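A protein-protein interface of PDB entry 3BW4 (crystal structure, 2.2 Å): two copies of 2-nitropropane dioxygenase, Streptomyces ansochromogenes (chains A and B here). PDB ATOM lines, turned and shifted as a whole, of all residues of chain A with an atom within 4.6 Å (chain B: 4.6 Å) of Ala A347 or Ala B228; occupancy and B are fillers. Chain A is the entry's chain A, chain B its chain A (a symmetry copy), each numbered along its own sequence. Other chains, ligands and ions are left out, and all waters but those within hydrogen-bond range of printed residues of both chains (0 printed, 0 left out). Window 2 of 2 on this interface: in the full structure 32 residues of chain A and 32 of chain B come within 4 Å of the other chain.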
ATOM      1  N   GLY A 221      -4.931  14.575  14.364  1.00  0.00           N
ATOM      2  CA  GLY A 221      -5.857  14.995  13.325  1.00  0.00           C
ATOM      3  C   GLY A 221      -5.490  16.348  12.739  1.00  0.00           C
ATOM      4  O   GLY A 221      -5.779  16.629  11.576  1.00  0.00           O
ATOM      5  N   ALA A 224      -2.834  15.745  10.252  1.00  0.00           N
ATOM      6  CA  ALA A 224      -3.432  15.271   9.008  1.00  0.00           C
ATOM      7  C   ALA A 224      -4.014  16.471   8.273  1.00  0.00           C
ATOM      8  O   ALA A 224      -3.940  16.564   7.040  1.00  0.00           O
ATOM      9  CB  ALA A 224      -4.536  14.263   9.302  1.00  0.00           C
ATOM     10  N   ALA A 225      -4.600  17.388   9.036  1.00  0.00           N
ATOM     11  CA  ALA A 225      -5.190  18.578   8.450  1.00  0.00           C
ATOM     12  C   ALA A 225      -4.165  19.398   7.665  1.00  0.00           C
ATOM     13  O   ALA A 225      -4.409  19.755   6.514  1.00  0.00           O
ATOM     14  CB  ALA A 225      -5.829  19.444   9.539  1.00  0.00           C
ATOM     15  N   GLU A 343      -3.192   8.958  16.148  1.00  0.00           N
ATOM     16  CA  GLU A 343      -4.261   9.901  15.847  1.00  0.00           C
ATOM     17  C   GLU A 343      -4.193  10.287  14.373  1.00  0.00           C
ATOM     18  O   GLU A 343      -5.218  10.386  13.699  1.00  0.00           O
ATOM     19  CB  GLU A 343      -4.135  11.142  16.733  1.00  0.00           C
ATOM     20  CG  GLU A 343      -4.501  10.885  18.187  1.00  0.00           C
ATOM     21  CD  GLU A 343      -4.182  12.059  19.093  1.00  0.00           C
ATOM     22  OE1 GLU A 343      -4.645  12.060  20.252  1.00  0.00           O
ATOM     23  OE2 GLU A 343      -3.461  12.977  18.658  1.00  0.00           O
ATOM     24  N   LEU A 344      -2.975  10.495  13.880  1.00  0.00           N
ATOM     25  CA  LEU A 344      -2.762  10.839  12.480  1.00  0.00           C
ATOM     26  C   LEU A 344      -3.332   9.733  11.596  1.00  0.00           C
ATOM     27  O   LEU A 344      -4.139   9.991  10.703  1.00  0.00           O
ATOM     28  CB  LEU A 344      -1.265  10.999  12.205  1.00  0.00           C
ATOM     29  CG  LEU A 344      -0.788  11.149  10.757  1.00  0.00           C
ATOM     30  CD1 LEU A 344      -1.469  12.335  10.103  1.00  0.00           C
ATOM     31  CD2 LEU A 344       0.723  11.339  10.743  1.00  0.00           C
ATOM     32  N   ALA A 345      -2.911   8.498  11.855  1.00  0.00           N
ATOM     33  CA  ALA A 345      -3.377   7.357  11.074  1.00  0.00           C
ATOM     34  C   ALA A 345      -4.900   7.298  11.081  1.00  0.00           C
ATOM     35  O   ALA A 345      -5.534   7.177  10.037  1.00  0.00           O
ATOM     36  CB  ALA A 345      -2.804   6.069  11.640  1.00  0.00           C
ATOM     37  N   GLU A 346      -5.477   7.392  12.272  1.00  0.00           N
ATOM     38  CA  GLU A 346      -6.922   7.351  12.433  1.00  0.00           C
ATOM     39  C   GLU A 346      -7.626   8.440  11.618  1.00  0.00           C
ATOM     40  O   GLU A 346      -8.687   8.204  11.039  1.00  0.00           O
ATOM     41  CB  GLU A 346      -7.277   7.497  13.910  1.00  0.00           C
ATOM     42  CG  GLU A 346      -8.751   7.711  14.176  1.00  0.00           C
ATOM     43  CD  GLU A 346      -9.033   8.042  15.628  1.00  0.00           C
ATOM     44  OE1 GLU A 346      -8.444   9.021  16.137  1.00  0.00           O
ATOM     45  OE2 GLU A 346      -9.845   7.327  16.256  1.00  0.00           O
ATOM     46  N   ALA A 347      -7.038   9.633  11.581  1.00  0.00           N
ATOM     47  CA  ALA A 347      -7.617  10.741  10.832  1.00  0.00           C
ATOM     48  C   ALA A 347      -7.514  10.486   9.332  1.00  0.00           C
ATOM     49  O   ALA A 347      -8.433  10.801   8.579  1.00  0.00           O
ATOM     50  CB  ALA A 347      -6.914  12.045  11.194  1.00  0.00           C
ATOM     51  N   ARG A 348      -6.391   9.922   8.899  1.00  0.00           N
ATOM     52  CA  ARG A 348      -6.192   9.616   7.483  1.00  0.00           C
ATOM     53  C   ARG A 348      -7.282   8.654   7.040  1.00  0.00           C
ATOM     54  O   ARG A 348      -7.988   8.892   6.059  1.00  0.00           O
ATOM     55  CB  ARG A 348      -4.838   8.944   7.254  1.00  0.00           C
ATOM     56  CG  ARG A 348      -3.633   9.862   7.245  1.00  0.00           C
ATOM     57  CD  ARG A 348      -2.359   9.023   7.126  1.00  0.00           C
ATOM     58  NE  ARG A 348      -1.163   9.823   6.885  1.00  0.00           N
ATOM     59  CZ  ARG A 348      -0.898  10.440   5.738  1.00  0.00           C
ATOM     60  NH1 ARG A 348      -1.746  10.348   4.724  1.00  0.00           N
ATOM     61  NH2 ARG A 348       0.218  11.145   5.603  1.00  0.00           N
ATOM     62  N   THR A 349      -7.403   7.555   7.776  1.00  0.00           N
ATOM     63  CA  THR A 349      -8.396   6.534   7.486  1.00  0.00           C
ATOM     64  C   THR A 349      -9.786   7.146   7.358  1.00  0.00           C
ATOM     65  O   THR A 349     -10.498   6.886   6.388  1.00  0.00           O
ATOM     66  CB  THR A 349      -8.410   5.460   8.593  1.00  0.00           C
ATOM     67  OG1 THR A 349      -7.136   4.806   8.634  1.00  0.00           O
ATOM     68  CG2 THR A 349      -9.492   4.428   8.326  1.00  0.00           C
ATOM     69  N   ALA A 350     -10.166   7.962   8.335  1.00  0.00           N
ATOM     70  CA  ALA A 350     -11.476   8.602   8.330  1.00  0.00           C
ATOM     71  C   ALA A 350     -11.691   9.428   7.068  1.00  0.00           C
ATOM     72  O   ALA A 350     -12.753   9.368   6.450  1.00  0.00           O
ATOM     73  CB  ALA A 350     -11.627   9.482   9.558  1.00  0.00           C
ATOM     74  N   LEU A 351     -10.676  10.193   6.686  1.00  0.00           N
ATOM     75  CA  LEU A 351     -10.750  11.040   5.499  1.00  0.00           C
ATOM     76  C   LEU A 351     -10.767  10.198   4.220  1.00  0.00           C
ATOM     77  O   LEU A 351     -10.601  10.721   3.117  1.00  0.00           O
ATOM     78  CB  LEU A 351      -9.559  12.005   5.476  1.00  0.00           C
ATOM     79  CG  LEU A 351      -9.585  13.160   4.470  1.00  0.00           C
ATOM     80  CD1 LEU A 351     -10.751  14.087   4.784  1.00  0.00           C
ATOM     81  CD2 LEU A 351      -8.269  13.924   4.532  1.00  0.00           C
ATOM     82  N   ALA B 224     -10.526  19.763   2.878  1.00  0.00           N
ATOM     83  CA  ALA B 224     -10.060  18.439   3.281  1.00  0.00           C
ATOM     84  C   ALA B 224      -9.381  18.568   4.637  1.00  0.00           C
ATOM     85  O   ALA B 224      -9.512  17.692   5.504  1.00  0.00           O
ATOM     86  CB  ALA B 224      -9.071  17.895   2.259  1.00  0.00           C
ATOM     87  N   ALA B 225      -8.647  19.662   4.816  1.00  0.00           N
ATOM     88  CA  ALA B 225      -7.953  19.896   6.070  1.00  0.00           C
ATOM     89  C   ALA B 225      -8.915  19.936   7.258  1.00  0.00           C
ATOM     90  O   ALA B 225      -8.694  19.253   8.256  1.00  0.00           O
ATOM     91  CB  ALA B 225      -7.155  21.200   5.997  1.00  0.00           C
ATOM     92  N   VAL B 226      -9.982  20.725   7.159  1.00  0.00           N
ATOM     93  CA  VAL B 226     -10.913  20.815   8.277  1.00  0.00           C
ATOM     94  C   VAL B 226     -11.668  19.516   8.529  1.00  0.00           C
ATOM     95  O   VAL B 226     -11.969  19.197   9.676  1.00  0.00           O
ATOM     96  CB  VAL B 226     -11.925  21.981   8.107  1.00  0.00           C
ATOM     97  CG1 VAL B 226     -11.166  23.295   7.969  1.00  0.00           C
ATOM     98  CG2 VAL B 226     -12.835  21.741   6.907  1.00  0.00           C
ATOM     99  N   LEU B 227     -11.963  18.767   7.470  1.00  0.00           N
ATOM    100  CA  LEU B 227     -12.667  17.501   7.632  1.00  0.00           C
ATOM    101  C   LEU B 227     -11.762  16.530   8.389  1.00  0.00           C
ATOM    102  O   LEU B 227     -12.225  15.763   9.236  1.00  0.00           O
ATOM    103  CB  LEU B 227     -13.037  16.897   6.274  1.00  0.00           C
ATOM    104  CG  LEU B 227     -14.000  17.679   5.372  1.00  0.00           C
ATOM    105  CD1 LEU B 227     -14.172  16.932   4.053  1.00  0.00           C
ATOM    106  CD2 LEU B 227     -15.341  17.860   6.065  1.00  0.00           C
ATOM    107  N   ALA B 228     -10.470  16.575   8.078  1.00  0.00           N
ATOM    108  CA  ALA B 228      -9.496  15.707   8.722  1.00  0.00           C
ATOM    109  C   ALA B 228      -9.391  16.047  10.202  1.00  0.00           C
ATOM    110  O   ALA B 228      -9.108  15.181  11.026  1.00  0.00           O
ATOM    111  CB  ALA B 228      -8.133  15.860   8.053  1.00  0.00           C
ATOM    112  N   ALA B 229      -9.622  17.313  10.534  1.00  0.00           N
ATOM    113  CA  ALA B 229      -9.546  17.761  11.918  1.00  0.00           C
ATOM    114  C   ALA B 229     -10.860  17.603  12.681  1.00  0.00           C
ATOM    115  O   ALA B 229     -10.983  18.093  13.802  1.00  0.00           O
ATOM    116  CB  ALA B 229      -9.088  19.209  11.972  1.00  0.00           C
ATOM    117  N   GLY B 230     -11.844  16.942  12.080  1.00  0.00           N
ATOM    118  CA  GLY B 230     -13.100  16.729  12.779  1.00  0.00           C
ATOM    119  C   GLY B 230     -14.352  17.445  12.297  1.00  0.00           C
ATOM    120  O   GLY B 230     -15.439  17.193  12.822  1.00  0.00           O
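Among the printed residues, pairs that only touch across the chains: Ala A225 with Ala B225, Gly A221 with Ala B228, Ala A347 with Ala B228, Leu A351 with Ala B224, Leu A351 with Leu B227, Gly A221 with Ala B229 and Ala A225 with Ala B228.
Arg A348 touches none of the printed residues of chain B.
Of the printed residues of chain B, Leu A351 touches Ala B224 and Leu B227.
Printed residues of chain A within 4 Å of Ala B224: Leu A351.
Of the printed residues of chain A, Ala B228 touches Gly A221 (3.7 Å), Ala A225 (3.97 Å) and Ala A347 (3.8 Å).
Of the printed residues of chain A, Ala B229 touches Gly A221 (3.9 Å).
Gly B230 touches none of the printed residues of chain A.
The nearest printed residue of chain B that does not touch Ala A347 is Ala B229 (6.0 Å).
Of the 12 printed residues of chain A, 4 touch a printed residue of chain B.
Along chain A the printed residues that touch a printed residue of chain B span positions 221 to 351.
Hydrophobic or aromatic side chains of chain B within 4 Å of the printed part of chain A: Ala B225, Leu B227 and Ala B228.
Among the printed residues, 7 pairs touch across the chains.
Ala B225 touches its own counterpart, Ala A225.
Positions printed for both chains: 224 and 225.
Of the 7 pairs that touch across the chains among the printed residues, 1 has its exchanged pair printed and touching as well.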
